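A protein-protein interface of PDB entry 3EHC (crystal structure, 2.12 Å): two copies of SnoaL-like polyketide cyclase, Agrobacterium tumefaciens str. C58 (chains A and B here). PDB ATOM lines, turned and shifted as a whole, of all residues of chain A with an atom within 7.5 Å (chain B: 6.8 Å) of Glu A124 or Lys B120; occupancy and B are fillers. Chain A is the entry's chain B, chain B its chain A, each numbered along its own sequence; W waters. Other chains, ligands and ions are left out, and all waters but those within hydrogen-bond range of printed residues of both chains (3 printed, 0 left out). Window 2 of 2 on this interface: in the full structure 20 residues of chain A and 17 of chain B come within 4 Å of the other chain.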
ATOM      1  N   MET A  87      -7.130 -24.737  13.087  1.00  0.00           N
ATOM      2  CA  MET A  87      -6.652 -23.851  12.023  1.00  0.00           C
ATOM      3  C   MET A  87      -5.402 -23.102  12.453  1.00  0.00           C
ATOM      4  O   MET A  87      -5.257 -21.917  12.177  1.00  0.00           O
ATOM      5  CB  MET A  87      -7.741 -22.895  11.590  1.00  0.00           C
ATOM      6  CG  MET A  87      -9.033 -23.600  11.166  1.00  0.00           C
ATOM      7  SD  MET A  87     -10.250 -22.329  10.285  1.00  0.00           S
ATOM      8  CE  MET A  87      -9.403 -22.419   8.491  1.00  0.00           C
ATOM      9  N   ASP A  88      -4.515 -23.834  13.136  1.00  0.00           N
ATOM     10  CA  ASP A  88      -3.283 -23.299  13.742  1.00  0.00           C
ATOM     11  C   ASP A  88      -3.455 -22.159  14.781  1.00  0.00           C
ATOM     12  O   ASP A  88      -2.529 -21.372  15.040  1.00  0.00           O
ATOM     13  CB  ASP A  88      -2.280 -23.004  12.626  1.00  0.00           C
ATOM     14  CG  ASP A  88      -2.020 -24.229  11.783  1.00  0.00           C
ATOM     15  OD1 ASP A  88      -1.547 -25.228  12.367  1.00  0.00           O
ATOM     16  OD2 ASP A  88      -2.320 -24.228  10.568  1.00  0.00           O
ATOM     17  N   LEU A  89      -4.640 -22.092  15.370  1.00  0.00           N
ATOM     18  CA  LEU A  89      -4.981 -21.100  16.361  1.00  0.00           C
ATOM     19  C   LEU A  89      -5.110 -21.801  17.717  1.00  0.00           C
ATOM     20  O   LEU A  89      -5.734 -22.854  17.792  1.00  0.00           O
ATOM     21  CB  LEU A  89      -6.316 -20.452  16.001  1.00  0.00           C
ATOM     22  CG  LEU A  89      -6.293 -19.632  14.720  1.00  0.00           C
ATOM     23  CD1 LEU A  89      -7.713 -19.100  14.377  1.00  0.00           C
ATOM     24  CD2 LEU A  89      -5.223 -18.519  14.880  1.00  0.00           C
ATOM     25  N   VAL A  91      -7.094 -22.166  20.191  1.00  0.00           N
ATOM     26  CA  VAL A  91      -8.439 -21.954  20.690  1.00  0.00           C
ATOM     27  C   VAL A  91      -8.574 -22.499  22.119  1.00  0.00           C
ATOM     28  O   VAL A  91      -9.128 -21.844  22.992  1.00  0.00           O
ATOM     29  CB  VAL A  91      -9.507 -22.580  19.785  1.00  0.00           C
ATOM     30  CG1 VAL A  91     -10.913 -22.386  20.379  1.00  0.00           C
ATOM     31  CG2 VAL A  91      -9.419 -21.946  18.404  1.00  0.00           C
ATOM     32  N   VAL A  96     -16.324 -20.781  20.132  1.00  0.00           N
ATOM     33  CA  VAL A  96     -16.135 -19.847  19.029  1.00  0.00           C
ATOM     34  C   VAL A  96     -17.204 -20.109  17.990  1.00  0.00           C
ATOM     35  O   VAL A  96     -17.721 -21.204  17.891  1.00  0.00           O
ATOM     36  CB  VAL A  96     -14.699 -19.949  18.399  1.00  0.00           C
ATOM     37  CG1 VAL A  96     -13.580 -19.371  19.365  1.00  0.00           C
ATOM     38  CG2 VAL A  96     -14.391 -21.381  17.971  1.00  0.00           C
ATOM     39  N   VAL A 117     -14.187 -23.572   2.242  1.00  0.00           N
ATOM     40  CA  VAL A 117     -13.425 -22.482   2.862  1.00  0.00           C
ATOM     41  C   VAL A 117     -14.052 -22.190   4.230  1.00  0.00           C
ATOM     42  O   VAL A 117     -15.259 -21.978   4.323  1.00  0.00           O
ATOM     43  CB  VAL A 117     -13.379 -21.199   1.935  1.00  0.00           C
ATOM     44  CG1 VAL A 117     -12.633 -20.127   2.589  1.00  0.00           C
ATOM     45  CG2 VAL A 117     -12.736 -21.509   0.584  1.00  0.00           C
ATOM     46  N   LEU A 118     -13.226 -22.195   5.281  1.00  0.00           N
ATOM     47  CA  LEU A 118     -13.634 -21.817   6.652  1.00  0.00           C
ATOM     48  C   LEU A 118     -13.234 -20.367   6.975  1.00  0.00           C
ATOM     49  O   LEU A 118     -12.237 -19.864   6.457  1.00  0.00           O
ATOM     50  CB  LEU A 118     -12.992 -22.765   7.677  1.00  0.00           C
ATOM     51  CG  LEU A 118     -13.529 -24.201   7.703  1.00  0.00           C
ATOM     52  CD1 LEU A 118     -12.452 -25.199   8.185  1.00  0.00           C
ATOM     53  CD2 LEU A 118     -14.748 -24.290   8.582  1.00  0.00           C
ATOM     54  N   ASP A 119     -14.035 -19.690   7.807  1.00  0.00           N
ATOM     55  CA  ASP A 119     -13.784 -18.307   8.173  1.00  0.00           C
ATOM     56  C   ASP A 119     -12.811 -18.240   9.368  1.00  0.00           C
ATOM     57  O   ASP A 119     -13.223 -18.069  10.525  1.00  0.00           O
ATOM     58  CB  ASP A 119     -15.106 -17.576   8.455  1.00  0.00           C
ATOM     59  CG  ASP A 119     -14.943 -16.054   8.570  1.00  0.00           C
ATOM     60  OD1 ASP A 119     -13.839 -15.526   8.341  1.00  0.00           O
ATOM     61  OD2 ASP A 119     -15.931 -15.390   8.906  1.00  0.00           O
ATOM     62  N   LYS A 120     -11.521 -18.343   9.045  1.00  0.00           N
ATOM     63  CA  LYS A 120     -10.446 -18.250   9.997  1.00  0.00           C
ATOM     64  C   LYS A 120     -10.392 -16.871  10.622  1.00  0.00           C
ATOM     65  O   LYS A 120     -10.107 -16.760  11.817  1.00  0.00           O
ATOM     66  CB  LYS A 120      -9.107 -18.639   9.345  1.00  0.00           C
ATOM     67  CG  LYS A 120      -7.910 -18.556  10.269  1.00  0.00           C
ATOM     68  CD  LYS A 120      -6.709 -19.335   9.808  1.00  0.00           C
ATOM     69  CE  LYS A 120      -5.579 -19.210  10.819  1.00  0.00           C
ATOM     70  NZ  LYS A 120      -4.361 -19.949  10.427  1.00  0.00           N
ATOM     71  N   VAL A 121     -10.685 -15.830   9.837  1.00  0.00           N
ATOM     72  CA  VAL A 121     -10.636 -14.459  10.341  1.00  0.00           C
ATOM     73  C   VAL A 121     -11.600 -14.269  11.532  1.00  0.00           C
ATOM     74  O   VAL A 121     -11.249 -13.576  12.452  1.00  0.00           O
ATOM     75  CB  VAL A 121     -10.838 -13.406   9.197  1.00  0.00           C
ATOM     76  CG1 VAL A 121     -10.761 -12.006   9.722  1.00  0.00           C
ATOM     77  CG2 VAL A 121      -9.753 -13.590   8.090  1.00  0.00           C
ATOM     78  N   ALA A 122     -12.792 -14.877  11.479  1.00  0.00           N
ATOM     79  CA  ALA A 122     -13.810 -14.813  12.548  1.00  0.00           C
ATOM     80  C   ALA A 122     -13.251 -15.379  13.844  1.00  0.00           C
ATOM     81  O   ALA A 122     -13.437 -14.806  14.916  1.00  0.00           O
ATOM     82  CB  ALA A 122     -15.111 -15.577  12.114  1.00  0.00           C
ATOM     83  N   ILE A 123     -12.523 -16.489  13.731  1.00  0.00           N
ATOM     84  CA  ILE A 123     -11.909 -17.116  14.899  1.00  0.00           C
ATOM     85  C   ILE A 123     -10.778 -16.236  15.473  1.00  0.00           C
ATOM     86  O   ILE A 123     -10.678 -16.065  16.679  1.00  0.00           O
ATOM     87  CB  ILE A 123     -11.368 -18.555  14.609  1.00  0.00           C
ATOM     88  CG1 ILE A 123     -12.449 -19.445  13.991  1.00  0.00           C
ATOM     89  CG2 ILE A 123     -10.807 -19.242  15.958  1.00  0.00           C
ATOM     90  CD1 ILE A 123     -11.901 -20.881  13.571  1.00  0.00           C
ATOM     91  N   GLU A 124      -9.921 -15.715  14.599  1.00  0.00           N
ATOM     92  CA  GLU A 124      -8.834 -14.816  14.993  1.00  0.00           C
ATOM     93  C   GLU A 124      -9.330 -13.634  15.807  1.00  0.00           C
ATOM     94  O   GLU A 124      -8.752 -13.290  16.852  1.00  0.00           O
ATOM     95  CB  GLU A 124      -8.056 -14.368  13.741  1.00  0.00           C
ATOM     96  CG  GLU A 124      -7.167 -15.454  13.160  1.00  0.00           C
ATOM     97  CD  GLU A 124      -6.568 -15.118  11.749  1.00  0.00           C
ATOM     98  OE1 GLU A 124      -6.981 -14.129  11.089  1.00  0.00           O
ATOM     99  OE2 GLU A 124      -5.665 -15.845  11.299  1.00  0.00           O
ATOM    100  N   ARG A 125     -10.390 -13.016  15.306  1.00  0.00           N
ATOM    101  CA  ARG A 125     -11.026 -11.924  16.000  1.00  0.00           C
ATOM    102  C   ARG A 125     -11.546 -12.263  17.368  1.00  0.00           C
ATOM    103  O   ARG A 125     -11.464 -11.441  18.247  1.00  0.00           O
ATOM    104  CB  ARG A 125     -12.181 -11.390  15.170  1.00  0.00           C
ATOM    105  CG  ARG A 125     -11.673 -10.544  14.086  1.00  0.00           C
ATOM    106  CD  ARG A 125     -12.782  -9.960  13.291  1.00  0.00           C
ATOM    107  NE  ARG A 125     -12.245  -9.430  12.041  1.00  0.00           N
ATOM    108  CZ  ARG A 125     -12.950  -9.314  10.924  1.00  0.00           C
ATOM    109  NH1 ARG A 125     -14.226  -9.711  10.901  1.00  0.00           N
ATOM    110  NH2 ARG A 125     -12.372  -8.808   9.829  1.00  0.00           N
ATOM    111  N   GLN A 126     -12.111 -13.455  17.530  1.00  0.00           N
ATOM    112  CA  GLN A 126     -12.628 -13.892  18.817  1.00  0.00           C
ATOM    113  C   GLN A 126     -11.547 -14.161  19.860  1.00  0.00           C
ATOM    114  O   GLN A 126     -11.793 -13.996  21.039  1.00  0.00           O
ATOM    115  CB  GLN A 126     -13.507 -15.119  18.634  1.00  0.00           C
ATOM    116  CG  GLN A 126     -14.822 -14.758  18.043  1.00  0.00           C
ATOM    117  CD  GLN A 126     -15.602 -15.944  17.503  1.00  0.00           C
ATOM    118  OE1 GLN A 126     -16.256 -16.688  18.257  1.00  0.00           O
ATOM    119  NE2 GLN A 126     -15.588 -16.091  16.187  1.00  0.00           N
ATOM    120  N   LEU A 127     -10.358 -14.570  19.413  1.00  0.00           N
ATOM    121  CA  LEU A 127      -9.233 -14.810  20.297  1.00  0.00           C
ATOM    122  C   LEU A 127      -8.396 -13.550  20.527  1.00  0.00           C
ATOM    123  O   LEU A 127      -7.583 -13.500  21.457  1.00  0.00           O
ATOM    124  CB  LEU A 127      -8.304 -15.906  19.716  1.00  0.00           C
ATOM    125  CG  LEU A 127      -8.888 -17.250  19.313  1.00  0.00           C
ATOM    126  CD1 LEU A 127      -7.758 -18.217  18.995  1.00  0.00           C
ATOM    127  CD2 LEU A 127      -9.841 -17.800  20.374  1.00  0.00           C
ATOM    128  N   GLY A 128      -8.587 -12.552  19.670  1.00  0.00           N
ATOM    129  CA  GLY A 128      -7.681 -11.419  19.559  1.00  0.00           C
ATOM    130  C   GLY A 128      -8.023 -10.185  20.366  1.00  0.00           C
ATOM    131  O   GLY A 128      -9.006 -10.039  21.066  1.00  0.00           O
ATOM    132  OXT GLY A 128      -7.265  -9.215  20.275  1.00  0.00           O
ATOM    133  N   PHE B  86      -2.728  -7.440   3.595  1.00  0.00           N
ATOM    134  CA  PHE B  86      -3.961  -7.966   3.030  1.00  0.00           C
ATOM    135  C   PHE B  86      -4.396  -9.101   3.971  1.00  0.00           C
ATOM    136  O   PHE B  86      -3.604 -10.039   4.234  1.00  0.00           O
ATOM    137  CB  PHE B  86      -3.733  -8.525   1.620  1.00  0.00           C
ATOM    138  CG  PHE B  86      -4.969  -9.124   1.009  1.00  0.00           C
ATOM    139  CD1 PHE B  86      -6.101  -8.355   0.832  1.00  0.00           C
ATOM    140  CD2 PHE B  86      -5.011 -10.465   0.650  1.00  0.00           C
ATOM    141  CE1 PHE B  86      -7.251  -8.911   0.295  1.00  0.00           C
ATOM    142  CE2 PHE B  86      -6.143 -11.009   0.110  1.00  0.00           C
ATOM    143  CZ  PHE B  86      -7.259 -10.240  -0.063  1.00  0.00           C
ATOM    144  N   MET B  87      -5.611  -8.997   4.493  1.00  0.00           N
ATOM    145  CA  MET B  87      -6.117  -9.925   5.530  1.00  0.00           C
ATOM    146  C   MET B  87      -5.132 -10.069   6.694  1.00  0.00           C
ATOM    147  O   MET B  87      -4.906 -11.183   7.203  1.00  0.00           O
ATOM    148  CB  MET B  87      -6.389 -11.306   4.955  1.00  0.00           C
ATOM    149  CG  MET B  87      -7.453 -11.264   3.840  1.00  0.00           C
ATOM    150  SD  MET B  87      -7.857 -13.083   3.288  1.00  0.00           S
ATOM    151  CE  MET B  87      -9.381 -13.222   4.612  1.00  0.00           C
ATOM    152  N   ASP B  88      -4.565  -8.931   7.099  1.00  0.00           N
ATOM    153  CA  ASP B  88      -3.534  -8.839   8.129  1.00  0.00           C
ATOM    154  C   ASP B  88      -2.312  -9.692   7.877  1.00  0.00           C
ATOM    155  O   ASP B  88      -1.648 -10.100   8.813  1.00  0.00           O
ATOM    156  CB  ASP B  88      -4.086  -9.154   9.520  1.00  0.00           C
ATOM    157  CG  ASP B  88      -5.155  -8.164   9.930  1.00  0.00           C
ATOM    158  OD1 ASP B  88      -4.758  -7.060  10.378  1.00  0.00           O
ATOM    159  OD2 ASP B  88      -6.365  -8.473   9.752  1.00  0.00           O
ATOM    160  N   LEU B  89      -2.006  -9.956   6.610  1.00  0.00           N
ATOM    161  CA  LEU B  89      -0.779 -10.662   6.271  1.00  0.00           C
ATOM    162  C   LEU B  89       0.107  -9.715   5.482  1.00  0.00           C
ATOM    163  O   LEU B  89      -0.370  -8.844   4.742  1.00  0.00           O
ATOM    164  CB  LEU B  89      -1.040 -11.983   5.509  1.00  0.00           C
ATOM    165  CG  LEU B  89      -1.988 -13.016   6.145  1.00  0.00           C
ATOM    166  CD1 LEU B  89      -2.437 -14.043   5.106  1.00  0.00           C
ATOM    167  CD2 LEU B  89      -1.365 -13.702   7.386  1.00  0.00           C
ATOM    168  N   PHE B  98      -5.879 -17.241  -4.405  1.00  0.00           N
ATOM    169  CA  PHE B  98      -6.831 -17.664  -3.372  1.00  0.00           C
ATOM    170  C   PHE B  98      -8.249 -17.558  -3.924  1.00  0.00           C
ATOM    171  O   PHE B  98      -8.500 -16.854  -4.899  1.00  0.00           O
ATOM    172  CB  PHE B  98      -6.688 -16.833  -2.118  1.00  0.00           C
ATOM    173  CG  PHE B  98      -6.921 -15.386  -2.347  1.00  0.00           C
ATOM    174  CD1 PHE B  98      -5.905 -14.587  -2.819  1.00  0.00           C
ATOM    175  CD2 PHE B  98      -8.173 -14.836  -2.162  1.00  0.00           C
ATOM    176  CE1 PHE B  98      -6.119 -13.255  -3.078  1.00  0.00           C
ATOM    177  CE2 PHE B  98      -8.376 -13.496  -2.412  1.00  0.00           C
ATOM    178  CZ  PHE B  98      -7.340 -12.717  -2.869  1.00  0.00           C
ATOM    179  N   CYS B  99      -9.170 -18.253  -3.283  1.00  0.00           N
ATOM    180  CA  CYS B  99     -10.565 -18.191  -3.639  1.00  0.00           C
ATOM    181  C   CYS B  99     -11.370 -17.497  -2.586  1.00  0.00           C
ATOM    182  O   CYS B  99     -10.950 -17.381  -1.444  1.00  0.00           O
ATOM    183  CB  CYS B  99     -11.123 -19.608  -3.824  1.00  0.00           C
ATOM    184  SG  CYS B  99     -10.349 -20.388  -5.244  1.00  0.00           S
ATOM    185  N   VAL B 117     -16.693 -15.449   2.358  1.00  0.00           N
ATOM    186  CA  VAL B 117     -15.537 -15.971   3.102  1.00  0.00           C
ATOM    187  C   VAL B 117     -14.367 -16.106   2.109  1.00  0.00           C
ATOM    188  O   VAL B 117     -14.552 -16.640   1.016  1.00  0.00           O
ATOM    189  CB  VAL B 117     -15.819 -17.302   3.850  1.00  0.00           C
ATOM    190  CG1 VAL B 117     -14.628 -17.730   4.608  1.00  0.00           C
ATOM    191  CG2 VAL B 117     -16.903 -17.134   4.872  1.00  0.00           C
ATOM    192  N   LEU B 118     -13.201 -15.550   2.467  1.00  0.00           N
ATOM    193  CA  LEU B 118     -11.971 -15.680   1.674  1.00  0.00           C
ATOM    194  C   LEU B 118     -11.029 -16.685   2.317  1.00  0.00           C
ATOM    195  O   LEU B 118     -10.996 -16.868   3.528  1.00  0.00           O
ATOM    196  CB  LEU B 118     -11.221 -14.360   1.456  1.00  0.00           C
ATOM    197  CG  LEU B 118     -11.862 -13.044   0.956  1.00  0.00           C
ATOM    198  CD1 LEU B 118     -10.723 -12.062   0.646  1.00  0.00           C
ATOM    199  CD2 LEU B 118     -12.807 -13.145  -0.261  1.00  0.00           C
ATOM    200  N   ASP B 119     -10.252 -17.352   1.469  1.00  0.00           N
ATOM    201  CA  ASP B 119      -9.335 -18.406   1.897  1.00  0.00           C
ATOM    202  C   ASP B 119      -7.985 -17.808   2.392  1.00  0.00           C
ATOM    203  O   ASP B 119      -6.980 -17.770   1.666  1.00  0.00           O
ATOM    204  CB  ASP B 119      -9.117 -19.370   0.725  1.00  0.00           C
ATOM    205  CG  ASP B 119      -8.469 -20.688   1.134  1.00  0.00           C
ATOM    206  OD1 ASP B 119      -8.073 -20.838   2.292  1.00  0.00           O
ATOM    207  OD2 ASP B 119      -8.359 -21.589   0.269  1.00  0.00           O
ATOM    208  N   LYS B 120      -7.981 -17.364   3.641  1.00  0.00           N
ATOM    209  CA  LYS B 120      -6.809 -16.822   4.273  1.00  0.00           C
ATOM    210  C   LYS B 120      -5.704 -17.865   4.369  1.00  0.00           C
ATOM    211  O   LYS B 120      -4.532 -17.556   4.251  1.00  0.00           O
ATOM    212  CB  LYS B 120      -7.162 -16.323   5.686  1.00  0.00           C
ATOM    213  CG  LYS B 120      -5.986 -15.703   6.395  1.00  0.00           C
ATOM    214  CD  LYS B 120      -6.353 -14.883   7.598  1.00  0.00           C
ATOM    215  CE  LYS B 120      -5.076 -14.328   8.270  1.00  0.00           C
ATOM    216  NZ  LYS B 120      -5.373 -13.372   9.353  1.00  0.00           N
ATOM    217  N   VAL B 121      -6.086 -19.109   4.608  1.00  0.00           N
ATOM    218  CA  VAL B 121      -5.129 -20.175   4.790  1.00  0.00           C
ATOM    219  C   VAL B 121      -4.260 -20.397   3.534  1.00  0.00           C
ATOM    220  O   VAL B 121      -3.051 -20.605   3.637  1.00  0.00           O
ATOM    221  CB  VAL B 121      -5.799 -21.517   5.223  1.00  0.00           C
ATOM    222  CG1 VAL B 121      -4.786 -22.647   5.176  1.00  0.00           C
ATOM    223  CG2 VAL B 121      -6.400 -21.401   6.624  1.00  0.00           C
ATOM    224  N   ALA B 122      -4.878 -20.320   2.357  1.00  0.00           N
ATOM    225  CA  ALA B 122      -4.138 -20.391   1.082  1.00  0.00           C
ATOM    226  C   ALA B 122      -3.048 -19.318   0.971  1.00  0.00           C
ATOM    227  O   ALA B 122      -1.910 -19.639   0.553  1.00  0.00           O
ATOM    228  CB  ALA B 122      -5.075 -20.301  -0.091  1.00  0.00           C
ATOM    229  N   ILE B 123      -3.355 -18.086   1.404  1.00  0.00           N
ATOM    230  CA  ILE B 123      -2.375 -16.984   1.391  1.00  0.00           C
ATOM    231  C   ILE B 123      -1.243 -17.238   2.397  1.00  0.00           C
ATOM    232  O   ILE B 123      -0.072 -17.101   2.059  1.00  0.00           O
ATOM    233  CB  ILE B 123      -3.012 -15.578   1.655  1.00  0.00           C
ATOM    234  CG1 ILE B 123      -4.214 -15.342   0.721  1.00  0.00           C
ATOM    235  CG2 ILE B 123      -1.907 -14.470   1.511  1.00  0.00           C
ATOM    236  CD1 ILE B 123      -4.864 -13.969   0.875  1.00  0.00           C
ATOM    237  N   GLU B 124      -1.597 -17.633   3.617  1.00  0.00           N
ATOM    238  CA  GLU B 124      -0.611 -18.035   4.621  1.00  0.00           C
ATOM    239  C   GLU B 124       0.398 -19.064   4.096  1.00  0.00           C
ATOM    240  O   GLU B 124       1.607 -18.938   4.330  1.00  0.00           O
ATOM    241  CB  GLU B 124      -1.303 -18.633   5.857  1.00  0.00           C
ATOM    242  CG  GLU B 124      -2.204 -17.616   6.566  1.00  0.00           C
ATOM    243  CD  GLU B 124      -2.823 -18.118   7.841  1.00  0.00           C
ATOM    244  OE1 GLU B 124      -3.184 -19.323   7.913  1.00  0.00           O
ATOM    245  OE2 GLU B 124      -2.953 -17.263   8.750  1.00  0.00           O
ATOM    246  N   ARG B 125      -0.104 -20.096   3.416  1.00  0.00           N
ATOM    247  CA  ARG B 125       0.734 -21.154   2.845  1.00  0.00           C
ATOM    248  C   ARG B 125       1.696 -20.614   1.827  1.00  0.00           C
ATOM    249  O   ARG B 125       2.847 -21.097   1.710  1.00  0.00           O
ATOM    250  CB  ARG B 125      -0.107 -22.233   2.160  1.00  0.00           C
ATOM    251  CG  ARG B 125      -0.403 -23.390   3.078  1.00  0.00           C
ATOM    252  CD  ARG B 125      -1.694 -24.129   2.767  1.00  0.00           C
ATOM    253  NE  ARG B 125      -2.125 -24.848   3.971  1.00  0.00           N
ATOM    254  CZ  ARG B 125      -3.223 -25.599   4.059  1.00  0.00           C
ATOM    255  NH1 ARG B 125      -4.016 -25.746   3.001  1.00  0.00           N
ATOM    256  NH2 ARG B 125      -3.526 -26.209   5.215  1.00  0.00           N
HETATM  257  O   HOH W   1     -10.409 -18.056   5.929  1.00  0.00           O
HETATM  258  O   HOH W   2     -11.553 -15.859   6.734  1.00  0.00           O
HETATM  259  O   HOH W   3      -9.087 -20.292   5.280  1.00  0.00           O
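Of the printed residues of chain B, Glu A124 touches Lys B120 and Glu B124. Of the printed residues of chain A, Leu B118 touches Val A117 (3.8 Å). Printed residues of chain B within 4 Å of Val A121: Met B87 (3.5 Å) and Lys B120 (3.7 Å). Of the printed residues of chain A, Met B87 touches Val A121. Of the printed residues of chain B, Met A87 touches Val B121 (3.7 Å). The nearest printed residue of chain B that does not touch Glu A124 is Met B87 (5.3 Å).
Water W1 lies within hydrogen-bond range of O of Leu A118 (2.6 Å), O of Leu B118 (2.7 Å), N of Lys A120 (3.3 Å) and N of Lys B120 (3.4 Å). Water W2 lies within hydrogen-bond range of OD1 of Asp A119 (2.8 Å), N of Val A121 (3.2 Å), N of Lys A120 (3.4 Å) and O of Leu B118 (3.4 Å). Water W3 lies within hydrogen-bond range of the side-chain carboxylate (OD1) of Asp B119 (3.2 Å), the backbone NH (N) of Val B121 (3.3 Å) and the backbone carbonyl oxygen (O) of Leu A118 (3.4 Å).
The side-chain amino group of Lys B120 lies within salt-bridge range of the side-chain carboxylate of Glu A124, at 2.5 Å. OE1 of Glu B124 lies within salt-bridge range of NZ of Lys A120 (2.8 Å).
NZ of Lys B120 sits at hydrogen-bond distance from O of Met B87 (3.1 Å). The backbone NH of Asp B119 lies within hydrogen-bond range of the backbone carbonyl oxygen of Cys B99 (3.0 Å). N of Ala B122 is in hydrogen-bond range of OD1 of Asp B119 (3.2 Å). NZ of Lys A120 sits at hydrogen-bond distance from O of Met A87, 2.8 Å away. OD1 of Asp A119 sits at hydrogen-bond distance from N of Ala A122 (3.4 Å).
CE of Met A87 touches CG2 of Val B121, 3.7 Å away. Val A117 touches Val B117 (CG1 to CG1, 3.7 Å). Leu B118 touches Val A117 (O to CG1, 3.8 Å). CG1 of Val A117 touches CA of Asp B119, at 3.8 Å. Leu A118 touches Val B117. CA of Asp A119 touches CG1 of Val B117, 3.7 Å away. CG2 of Val B121 touches CD of Lys A120, 3.8 Å away. Val A121 touches Met B87 (CG2 to CE, 3.5 Å). Val A121 touches Lys B120 (CG2 to CD, 3.7 Å). Glu A124 touches Glu B124 (OE2 to OE2, 3.98 Å).
Of the 15 printed residues of chain B, 7 touch a printed residue of chain A. Hydrophobic or aromatic side chains of chain B within 4 Å of the printed part of chain A: Met B87, Val B117 and Val B121. Of the 17 printed residues of chain A, 7 touch a printed residue of chain B. Hydrophobic or aromatic side chains of chain A that line the printed part of chain B: Met A87, Val A117 and Val A121.
Met A87 touches Val B121, and with the chains exchanged Val A121 touches Met B87. Lys A120 touches Val B121, and with the chains exchanged Val A121 touches Lys B120. Lys A120 touches Glu B124, and with the chains exchanged Glu A124 touches Lys B120. Glu A124 touches its own counterpart, Glu B124. Of the 12 pairs that touch across the chains among the printed residues, 12 have their exchanged pair printed and touching as well.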
